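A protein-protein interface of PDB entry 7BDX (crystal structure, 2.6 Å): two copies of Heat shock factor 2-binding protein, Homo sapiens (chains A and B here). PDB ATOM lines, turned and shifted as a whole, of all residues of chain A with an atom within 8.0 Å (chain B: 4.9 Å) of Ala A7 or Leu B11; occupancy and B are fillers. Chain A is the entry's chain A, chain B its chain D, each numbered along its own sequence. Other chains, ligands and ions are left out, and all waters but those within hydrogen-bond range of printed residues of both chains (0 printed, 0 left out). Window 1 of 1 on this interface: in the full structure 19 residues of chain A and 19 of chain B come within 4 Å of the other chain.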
ATOM      1  N   ALA A   1     -28.900  20.258 -30.576  1.00  0.00           N
ATOM      2  CA  ALA A   1     -29.463  19.251 -29.685  1.00  0.00           C
ATOM      3  C   ALA A   1     -28.466  18.693 -28.684  1.00  0.00           C
ATOM      4  O   ALA A   1     -28.508  19.029 -27.495  1.00  0.00           O
ATOM      5  N   GLU A   2     -27.574  17.803 -29.152  1.00  0.00           N
ATOM      6  CA  GLU A   2     -26.543  17.240 -28.280  1.00  0.00           C
ATOM      7  C   GLU A   2     -25.393  18.263 -28.179  1.00  0.00           C
ATOM      8  O   GLU A   2     -24.881  18.515 -27.087  1.00  0.00           O
ATOM      9  CB  GLU A   2     -26.043  15.875 -28.831  1.00  0.00           C
ATOM     10  CG  GLU A   2     -24.928  15.243 -28.012  1.00  0.00           C
ATOM     11  CD  GLU A   2     -24.155  14.091 -28.642  1.00  0.00           C
ATOM     12  OE1 GLU A   2     -23.028  13.802 -28.176  1.00  0.00           O
ATOM     13  OE2 GLU A   2     -24.662  13.489 -29.617  1.00  0.00           O
ATOM     14  N   MET A   3     -24.995  18.832 -29.336  1.00  0.00           N
ATOM     15  CA  MET A   3     -23.932  19.815 -29.457  1.00  0.00           C
ATOM     16  C   MET A   3     -24.298  21.119 -28.748  1.00  0.00           C
ATOM     17  O   MET A   3     -23.442  21.728 -28.098  1.00  0.00           O
ATOM     18  CB  MET A   3     -23.610  20.069 -30.939  1.00  0.00           C
ATOM     19  CG  MET A   3     -22.646  21.236 -31.200  1.00  0.00           C
ATOM     20  SD  MET A   3     -21.055  21.350 -30.055  1.00  0.00           S
ATOM     21  CE  MET A   3     -19.872  21.014 -31.347  1.00  0.00           C
ATOM     22  N   GLY A   4     -25.559  21.524 -28.861  1.00  0.00           N
ATOM     23  CA  GLY A   4     -26.041  22.732 -28.210  1.00  0.00           C
ATOM     24  C   GLY A   4     -25.927  22.659 -26.700  1.00  0.00           C
ATOM     25  O   GLY A   4     -25.455  23.605 -26.067  1.00  0.00           O
ATOM     26  N   ALA A   5     -26.334  21.528 -26.113  1.00  0.00           N
ATOM     27  CA  ALA A   5     -26.270  21.356 -24.668  1.00  0.00           C
ATOM     28  C   ALA A   5     -24.845  21.202 -24.154  1.00  0.00           C
ATOM     29  O   ALA A   5     -24.568  21.591 -23.023  1.00  0.00           O
ATOM     30  CB  ALA A   5     -27.096  20.162 -24.244  1.00  0.00           C
ATOM     31  N   ALA A   6     -23.943  20.632 -24.963  1.00  0.00           N
ATOM     32  CA  ALA A   6     -22.550  20.456 -24.562  1.00  0.00           C
ATOM     33  C   ALA A   6     -21.847  21.811 -24.432  1.00  0.00           C
ATOM     34  O   ALA A   6     -21.060  22.016 -23.504  1.00  0.00           O
ATOM     35  CB  ALA A   6     -21.829  19.592 -25.582  1.00  0.00           C
ATOM     36  N   ALA A   7     -22.153  22.739 -25.363  1.00  0.00           N
ATOM     37  CA  ALA A   7     -21.590  24.085 -25.380  1.00  0.00           C
ATOM     38  C   ALA A   7     -22.142  24.908 -24.218  1.00  0.00           C
ATOM     39  O   ALA A   7     -21.395  25.645 -23.570  1.00  0.00           O
ATOM     40  CB  ALA A   7     -21.893  24.764 -26.708  1.00  0.00           C
ATOM     41  N   CYS A   8     -23.442  24.759 -23.940  1.00  0.00           N
ATOM     42  CA  CYS A   8     -24.126  25.436 -22.843  1.00  0.00           C
ATOM     43  C   CYS A   8     -23.618  24.956 -21.489  1.00  0.00           C
ATOM     44  O   CYS A   8     -23.494  25.748 -20.558  1.00  0.00           O
ATOM     45  CB  CYS A   8     -25.630  25.254 -22.966  1.00  0.00           C
ATOM     46  SG  CYS A   8     -26.425  26.474 -24.034  1.00  0.00           S
ATOM     47  N   THR A   9     -23.342  23.658 -21.373  1.00  0.00           N
ATOM     48  CA  THR A   9     -22.797  23.091 -20.144  1.00  0.00           C
ATOM     49  C   THR A   9     -21.381  23.620 -19.907  1.00  0.00           C
ATOM     50  O   THR A   9     -21.019  23.943 -18.778  1.00  0.00           O
ATOM     51  CB  THR A   9     -22.859  21.564 -20.190  1.00  0.00           C
ATOM     52  OG1 THR A   9     -24.207  21.188 -20.459  1.00  0.00           O
ATOM     53  CG2 THR A   9     -22.415  20.932 -18.900  1.00  0.00           C
ATOM     54  N   LEU A  10     -20.605  23.759 -20.980  1.00  0.00           N
ATOM     55  CA  LEU A  10     -19.253  24.277 -20.896  1.00  0.00           C
ATOM     56  C   LEU A  10     -19.270  25.735 -20.420  1.00  0.00           C
ATOM     57  O   LEU A  10     -18.470  26.107 -19.567  1.00  0.00           O
ATOM     58  CB  LEU A  10     -18.562  24.127 -22.273  1.00  0.00           C
ATOM     59  CG  LEU A  10     -17.043  24.348 -22.325  1.00  0.00           C
ATOM     60  CD1 LEU A  10     -16.331  23.549 -21.249  1.00  0.00           C
ATOM     61  CD2 LEU A  10     -16.485  24.007 -23.708  1.00  0.00           C
ATOM     62  N   LEU A  11     -20.217  26.526 -20.939  1.00  0.00           N
ATOM     63  CA  LEU A  11     -20.428  27.920 -20.599  1.00  0.00           C
ATOM     64  C   LEU A  11     -20.895  28.095 -19.137  1.00  0.00           C
ATOM     65  O   LEU A  11     -20.513  29.060 -18.481  1.00  0.00           O
ATOM     66  CB  LEU A  11     -21.442  28.502 -21.577  1.00  0.00           C
ATOM     67  CG  LEU A  11     -21.504  30.006 -21.694  1.00  0.00           C
ATOM     68  CD1 LEU A  11     -20.125  30.627 -21.906  1.00  0.00           C
ATOM     69  CD2 LEU A  11     -22.441  30.415 -22.786  1.00  0.00           C
ATOM     70  N   TRP A  12     -21.705  27.155 -18.628  1.00  0.00           N
ATOM     71  CA  TRP A  12     -22.188  27.102 -17.240  1.00  0.00           C
ATOM     72  C   TRP A  12     -20.986  26.890 -16.285  1.00  0.00           C
ATOM     73  O   TRP A  12     -20.923  27.491 -15.208  1.00  0.00           O
ATOM     74  CB  TRP A  12     -23.174  25.925 -17.117  1.00  0.00           C
ATOM     75  CG  TRP A  12     -23.892  25.770 -15.810  1.00  0.00           C
ATOM     76  CD1 TRP A  12     -23.905  26.636 -14.757  1.00  0.00           C
ATOM     77  CD2 TRP A  12     -24.758  24.686 -15.449  1.00  0.00           C
ATOM     78  NE1 TRP A  12     -24.707  26.144 -13.750  1.00  0.00           N
ATOM     79  CE2 TRP A  12     -25.251  24.952 -14.157  1.00  0.00           C
ATOM     80  CE3 TRP A  12     -25.135  23.499 -16.078  1.00  0.00           C
ATOM     81  CZ2 TRP A  12     -26.109  24.082 -13.500  1.00  0.00           C
ATOM     82  CZ3 TRP A  12     -26.015  22.658 -15.440  1.00  0.00           C
ATOM     83  CH2 TRP A  12     -26.467  22.935 -14.155  1.00  0.00           C
ATOM     84  N   GLY A  13     -20.047  26.047 -16.701  1.00  0.00           N
ATOM     85  CA  GLY A  13     -18.846  25.775 -15.937  1.00  0.00           C
ATOM     86  C   GLY A  13     -17.944  26.981 -15.823  1.00  0.00           C
ATOM     87  O   GLY A  13     -17.508  27.312 -14.725  1.00  0.00           O
ATOM     88  N   VAL A  14     -17.678  27.671 -16.943  1.00  0.00           N
ATOM     89  CA  VAL A  14     -16.808  28.844 -16.921  1.00  0.00           C
ATOM     90  C   VAL A  14     -17.506  30.099 -16.383  1.00  0.00           C
ATOM     91  O   VAL A  14     -16.826  31.012 -15.916  1.00  0.00           O
ATOM     92  CB  VAL A  14     -16.132  29.099 -18.278  1.00  0.00           C
ATOM     93  CG1 VAL A  14     -15.324  27.890 -18.706  1.00  0.00           C
ATOM     94  CG2 VAL A  14     -17.157  29.462 -19.341  1.00  0.00           C
ATOM     95  N   SER A  15     -18.851  30.138 -16.394  1.00  0.00           N
ATOM     96  CA  SER A  15     -19.605  31.297 -15.888  1.00  0.00           C
ATOM     97  C   SER A  15     -19.498  31.521 -14.367  1.00  0.00           C
ATOM     98  O   SER A  15     -19.969  32.537 -13.861  1.00  0.00           O
ATOM     99  CB  SER A  15     -21.062  31.234 -16.318  1.00  0.00           C
ATOM    100  OG  SER A  15     -21.669  30.087 -15.752  1.00  0.00           O
ATOM    101  N   VAL A  20     -15.471  36.003 -16.750  1.00  0.00           N
ATOM    102  CA  VAL A  20     -16.276  35.425 -17.811  1.00  0.00           C
ATOM    103  C   VAL A  20     -17.647  36.081 -17.844  1.00  0.00           C
ATOM    104  O   VAL A  20     -18.158  36.362 -18.922  1.00  0.00           O
ATOM    105  CB  VAL A  20     -16.369  33.897 -17.641  1.00  0.00           C
ATOM    106  CG1 VAL A  20     -17.237  33.273 -18.717  1.00  0.00           C
ATOM    107  CG2 VAL A  20     -14.984  33.285 -17.660  1.00  0.00           C
ATOM    108  N   ILE A  24     -19.612  38.091 -20.909  1.00  0.00           N
ATOM    109  CA  ILE A  24     -20.890  37.635 -21.462  1.00  0.00           C
ATOM    110  C   ILE A  24     -21.880  38.809 -21.666  1.00  0.00           C
ATOM    111  O   ILE A  24     -22.731  38.764 -22.570  1.00  0.00           O
ATOM    112  CB  ILE A  24     -21.488  36.511 -20.549  1.00  0.00           C
ATOM    113  CG1 ILE A  24     -20.725  35.194 -20.721  1.00  0.00           C
ATOM    114  CG2 ILE A  24     -22.988  36.287 -20.780  1.00  0.00           C
ATOM    115  CD1 ILE A  24     -21.082  34.141 -19.738  1.00  0.00           C
ATOM    116  N   LEU A  31     -25.791  38.966 -30.422  1.00  0.00           N
ATOM    117  CA  LEU A  31     -26.626  37.755 -30.311  1.00  0.00           C
ATOM    118  C   LEU A  31     -27.399  37.986 -29.060  1.00  0.00           C
ATOM    119  O   LEU A  31     -26.767  38.101 -28.015  1.00  0.00           O
ATOM    120  CB  LEU A  31     -25.812  36.446 -30.118  1.00  0.00           C
ATOM    121  CG  LEU A  31     -24.329  36.553 -29.775  1.00  0.00           C
ATOM    122  CD1 LEU A  31     -24.011  35.949 -28.428  1.00  0.00           C
ATOM    123  CD2 LEU A  31     -23.519  35.936 -30.850  1.00  0.00           C
ATOM    124  N   PHE A  33     -28.429  36.793 -26.341  1.00  0.00           N
ATOM    125  CA  PHE A  33     -28.266  35.586 -25.534  1.00  0.00           C
ATOM    126  C   PHE A  33     -29.335  35.422 -24.449  1.00  0.00           C
ATOM    127  O   PHE A  33     -29.946  34.364 -24.368  1.00  0.00           O
ATOM    128  CB  PHE A  33     -26.855  35.507 -24.943  1.00  0.00           C
ATOM    129  CG  PHE A  33     -26.607  34.276 -24.105  1.00  0.00           C
ATOM    130  CD1 PHE A  33     -26.208  33.089 -24.688  1.00  0.00           C
ATOM    131  CD2 PHE A  33     -26.744  34.316 -22.729  1.00  0.00           C
ATOM    132  CE1 PHE A  33     -25.953  31.969 -23.911  1.00  0.00           C
ATOM    133  CE2 PHE A  33     -26.514  33.187 -21.960  1.00  0.00           C
ATOM    134  CZ  PHE A  33     -26.127  32.020 -22.558  1.00  0.00           C
ATOM    135  N   PHE A  62     -29.716  21.113 -21.406  1.00  0.00           N
ATOM    136  CA  PHE A  62     -29.570  22.353 -22.156  1.00  0.00           C
ATOM    137  C   PHE A  62     -30.210  23.479 -21.336  1.00  0.00           C
ATOM    138  O   PHE A  62     -29.587  24.520 -21.125  1.00  0.00           O
ATOM    139  CB  PHE A  62     -30.265  22.230 -23.537  1.00  0.00           C
ATOM    140  CG  PHE A  62     -29.818  23.200 -24.611  1.00  0.00           C
ATOM    141  CD1 PHE A  62     -29.547  24.527 -24.310  1.00  0.00           C
ATOM    142  CD2 PHE A  62     -29.711  22.796 -25.925  1.00  0.00           C
ATOM    143  CE1 PHE A  62     -29.132  25.412 -25.294  1.00  0.00           C
ATOM    144  CE2 PHE A  62     -29.306  23.687 -26.910  1.00  0.00           C
ATOM    145  CZ  PHE A  62     -29.011  24.987 -26.586  1.00  0.00           C
ATOM    146  N   ALA A  65     -28.410  24.170 -18.062  1.00  0.00           N
ATOM    147  CA  ALA A  65     -27.250  24.977 -18.331  1.00  0.00           C
ATOM    148  C   ALA A  65     -27.656  26.425 -18.494  1.00  0.00           C
ATOM    149  O   ALA A  65     -27.009  27.290 -17.919  1.00  0.00           O
ATOM    150  CB  ALA A  65     -26.559  24.465 -19.569  1.00  0.00           C
ATOM    151  N   ILE A  69     -26.489  29.307 -16.043  1.00  0.00           N
ATOM    152  CA  ILE A  69     -25.755  30.469 -16.533  1.00  0.00           C
ATOM    153  C   ILE A  69     -26.446  31.731 -16.037  1.00  0.00           C
ATOM    154  O   ILE A  69     -25.772  32.592 -15.480  1.00  0.00           O
ATOM    155  CB  ILE A  69     -25.598  30.466 -18.077  1.00  0.00           C
ATOM    156  CG1 ILE A  69     -24.831  29.218 -18.563  1.00  0.00           C
ATOM    157  CG2 ILE A  69     -24.920  31.749 -18.566  1.00  0.00           C
ATOM    158  CD1 ILE A  69     -24.891  28.982 -20.058  1.00  0.00           C
ATOM    159  N   ALA B   7     -24.299  30.574 -27.856  1.00  0.00           N
ATOM    160  CA  ALA B   7     -23.518  30.021 -26.761  1.00  0.00           C
ATOM    161  C   ALA B   7     -22.081  29.751 -27.205  1.00  0.00           C
ATOM    162  O   ALA B   7     -21.136  30.009 -26.450  1.00  0.00           O
ATOM    163  CB  ALA B   7     -24.166  28.735 -26.266  1.00  0.00           C
ATOM    164  N   CYS B   8     -21.916  29.243 -28.438  1.00  0.00           N
ATOM    165  CA  CYS B   8     -20.615  28.967 -29.044  1.00  0.00           C
ATOM    166  C   CYS B   8     -19.838  30.234 -29.299  1.00  0.00           C
ATOM    167  O   CYS B   8     -18.630  30.250 -29.107  1.00  0.00           O
ATOM    168  CB  CYS B   8     -20.779  28.153 -30.318  1.00  0.00           C
ATOM    169  SG  CYS B   8     -20.855  26.366 -30.031  1.00  0.00           S
ATOM    170  N   THR B   9     -20.522  31.293 -29.724  1.00  0.00           N
ATOM    171  CA  THR B   9     -19.888  32.578 -29.972  1.00  0.00           C
ATOM    172  C   THR B   9     -19.409  33.187 -28.665  1.00  0.00           C
ATOM    173  O   THR B   9     -18.306  33.715 -28.624  1.00  0.00           O
ATOM    174  CB  THR B   9     -20.849  33.509 -30.720  1.00  0.00           C
ATOM    175  OG1 THR B   9     -21.264  32.861 -31.917  1.00  0.00           O
ATOM    176  CG2 THR B   9     -20.213  34.845 -31.063  1.00  0.00           C
ATOM    177  N   LEU B  10     -20.202  33.082 -27.582  1.00  0.00           N
ATOM    178  CA  LEU B  10     -19.772  33.591 -26.279  1.00  0.00           C
ATOM    179  C   LEU B  10     -18.537  32.839 -25.810  1.00  0.00           C
ATOM    180  O   LEU B  10     -17.566  33.460 -25.405  1.00  0.00           O
ATOM    181  CB  LEU B  10     -20.883  33.457 -25.228  1.00  0.00           C
ATOM    182  CG  LEU B  10     -22.001  34.498 -25.242  1.00  0.00           C
ATOM    183  CD1 LEU B  10     -22.887  34.335 -24.023  1.00  0.00           C
ATOM    184  CD2 LEU B  10     -21.451  35.929 -25.264  1.00  0.00           C
ATOM    185  N   LEU B  11     -18.544  31.511 -25.956  1.00  0.00           N
ATOM    186  CA  LEU B  11     -17.437  30.637 -25.569  1.00  0.00           C
ATOM    187  C   LEU B  11     -16.164  30.976 -26.325  1.00  0.00           C
ATOM    188  O   LEU B  11     -15.092  30.917 -25.742  1.00  0.00           O
ATOM    189  CB  LEU B  11     -17.818  29.175 -25.813  1.00  0.00           C
ATOM    190  CG  LEU B  11     -18.237  28.288 -24.650  1.00  0.00           C
ATOM    191  CD1 LEU B  11     -18.423  26.886 -25.144  1.00  0.00           C
ATOM    192  CD2 LEU B  11     -17.248  28.324 -23.527  1.00  0.00           C
ATOM    193  N   TRP B  12     -16.280  31.336 -27.620  1.00  0.00           N
ATOM    194  CA  TRP B  12     -15.182  31.772 -28.507  1.00  0.00           C
ATOM    195  C   TRP B  12     -14.564  33.080 -27.966  1.00  0.00           C
ATOM    196  O   TRP B  12     -13.342  33.259 -27.979  1.00  0.00           O
ATOM    197  CB  TRP B  12     -15.748  32.016 -29.918  1.00  0.00           C
ATOM    198  CG  TRP B  12     -14.751  32.326 -30.999  1.00  0.00           C
ATOM    199  CD1 TRP B  12     -13.388  32.240 -30.925  1.00  0.00           C
ATOM    200  CD2 TRP B  12     -15.056  32.700 -32.353  1.00  0.00           C
ATOM    201  NE1 TRP B  12     -12.827  32.566 -32.141  1.00  0.00           N
ATOM    202  CE2 TRP B  12     -13.828  32.839 -33.039  1.00  0.00           C
ATOM    203  CE3 TRP B  12     -16.248  32.961 -33.044  1.00  0.00           C
ATOM    204  CZ2 TRP B  12     -13.760  33.188 -34.385  1.00  0.00           C
ATOM    205  CZ3 TRP B  12     -16.175  33.280 -34.384  1.00  0.00           C
ATOM    206  CH2 TRP B  12     -14.940  33.407 -35.037  1.00  0.00           C
ATOM    207  N   GLY B  13     -15.416  33.977 -27.498  1.00  0.00           N
ATOM    208  CA  GLY B  13     -14.986  35.237 -26.940  1.00  0.00           C
ATOM    209  C   GLY B  13     -14.200  35.064 -25.666  1.00  0.00           C
ATOM    210  O   GLY B  13     -13.120  35.640 -25.528  1.00  0.00           O
ATOM    211  N   VAL B  14     -14.712  34.254 -24.739  1.00  0.00           N
ATOM    212  CA  VAL B  14     -14.041  34.056 -23.455  1.00  0.00           C
ATOM    213  C   VAL B  14     -12.839  33.110 -23.549  1.00  0.00           C
ATOM    214  O   VAL B  14     -11.937  33.205 -22.717  1.00  0.00           O
ATOM    215  CB  VAL B  14     -15.026  33.641 -22.335  1.00  0.00           C
ATOM    216  CG1 VAL B  14     -16.133  34.681 -22.189  1.00  0.00           C
ATOM    217  CG2 VAL B  14     -15.610  32.252 -22.605  1.00  0.00           C
ATOM    218  N   SER B  15     -12.799  32.234 -24.571  1.00  0.00           N
ATOM    219  CA  SER B  15     -11.703  31.280 -24.756  1.00  0.00           C
ATOM    220  C   SER B  15     -10.360  31.921 -25.093  1.00  0.00           C
ATOM    221  O   SER B  15      -9.357  31.222 -25.125  1.00  0.00           O
ATOM    222  CB  SER B  15     -12.063  30.230 -25.800  1.00  0.00           C
ATOM    223  OG  SER B  15     -12.254  30.834 -27.066  1.00  0.00           O
ATOM    224  N   ILE B  24     -11.938  25.053 -18.906  1.00  0.00           N
ATOM    225  CA  ILE B  24     -12.671  24.254 -19.885  1.00  0.00           C
ATOM    226  C   ILE B  24     -12.165  22.827 -19.857  1.00  0.00           C
ATOM    227  O   ILE B  24     -12.964  21.911 -19.735  1.00  0.00           O
ATOM    228  CB  ILE B  24     -12.581  24.894 -21.296  1.00  0.00           C
ATOM    229  CG1 ILE B  24     -13.516  26.109 -21.403  1.00  0.00           C
ATOM    230  CG2 ILE B  24     -12.867  23.885 -22.419  1.00  0.00           C
ATOM    231  CD1 ILE B  24     -13.161  27.050 -22.489  1.00  0.00           C
ATOM    232  N   PHE B  33     -17.626  17.720 -25.802  1.00  0.00           N
ATOM    233  CA  PHE B  33     -17.603  18.919 -26.637  1.00  0.00           C
ATOM    234  C   PHE B  33     -16.643  18.833 -27.832  1.00  0.00           C
ATOM    235  O   PHE B  33     -17.070  19.094 -28.952  1.00  0.00           O
ATOM    236  CB  PHE B  33     -17.328  20.182 -25.801  1.00  0.00           C
ATOM    237  CG  PHE B  33     -17.360  21.433 -26.639  1.00  0.00           C
ATOM    238  CD1 PHE B  33     -18.553  21.904 -27.155  1.00  0.00           C
ATOM    239  CD2 PHE B  33     -16.194  22.090 -26.977  1.00  0.00           C
ATOM    240  CE1 PHE B  33     -18.575  23.017 -27.972  1.00  0.00           C
ATOM    241  CE2 PHE B  33     -16.218  23.194 -27.811  1.00  0.00           C
ATOM    242  CZ  PHE B  33     -17.409  23.654 -28.296  1.00  0.00           C
ATOM    243  N   ILE B  69     -12.826  28.354 -31.242  1.00  0.00           N
ATOM    244  CA  ILE B  69     -12.592  27.801 -29.917  1.00  0.00           C
ATOM    245  C   ILE B  69     -11.440  26.807 -29.980  1.00  0.00           C
ATOM    246  O   ILE B  69     -10.518  26.915 -29.173  1.00  0.00           O
ATOM    247  CB  ILE B  69     -13.865  27.173 -29.298  1.00  0.00           C
ATOM    248  CG1 ILE B  69     -14.982  28.204 -29.155  1.00  0.00           C
ATOM    249  CG2 ILE B  69     -13.557  26.531 -27.935  1.00  0.00           C
ATOM    250  CD1 ILE B  69     -16.305  27.604 -28.838  1.00  0.00           C
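SG of Cys A8 sits close to O of Gly A4 (3.6 Å).
The side-chain hydroxyl of Ser A15 lies close to the backbone carbonyl oxygen of Leu A11 (3.1 Å).
OG of Ser B15 sits close to O of Leu B11 (3.1 Å).
Among the printed residues, merely in contact across the chains: Leu A31 with Thr B9 (3.5 Å), Ala A7 with Leu B11 (3.6 Å), Phe A33 with Leu B10 (3.6 Å), Met A3 with Phe B33 (3.6 Å), Leu A10 with Ile B24 (3.7 Å), Val A14 with Ile B24 (3.7 Å), Leu A10 with Leu B11 (3.8 Å), Ile A24 with Leu B10 (3.8 Å), Leu A10 with Phe B33 (3.8 Å), Ala A7 with Cys B8 (3.8 Å), Cys A8 with Ala B7 (3.9 Å), Val A20 with Val B14 (3.9 Å), Leu A11 with Ala B7 (3.9 Å) and Ala A7 with Phe B33 (3.96 Å).
Ala A7 touches just these residues of chain B: Cys B8, Leu B11 and Phe B33.
Leu B11 touches just these residues of chain A: Ala A7 and Leu A10.
Of the printed residues of chain A, Cys B8 touches Ala A7 (3.8 Å).
Of the printed residues of chain B, Leu A10 touches Leu B11 (3.8 Å), Ile B24 (3.7 Å) and Phe B33 (3.8 Å).
Printed residues of chain B within 4 Å of Phe A33: Leu B10 (3.6 Å).
Printed residues of chain B within 4 Å of Cys A8: Ala B7.
Of the printed residues of chain B, Val A14 touches Ile B24.
The nearest residue of chain A that does not touch Leu B11 is Leu A11 (4.03 Å).
The nearest printed residue of chain B that does not touch Met A3 is Cys B8 (5.0 Å).
Of the 12 printed residues of chain B, 8 touch a printed residue of chain A.
Hydrophobic or aromatic side chains of chain A that line the printed part of chain B: Met A3, Ala A7, Leu A10, Leu A11, Val A14, Val A20, Ile A24, Leu A31 and Phe A33.
Among the printed residues, no Asp or Glu carboxylate lies within 4 Å of a Lys or Arg side-chain nitrogen of the other chain.
Ala A7 touches Cys B8, and with the chains exchanged Cys A8 touches Ala B7.
Ala A7 touches Leu B11, and with the chains exchanged Leu A11 touches Ala B7.
Leu A10 touches Leu B11, but with the chains exchanged Leu A11 does not touch Leu B10 (4.1 Å).
Leu A10 touches Phe B33, and with the chains exchanged Phe A33 touches Leu B10.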
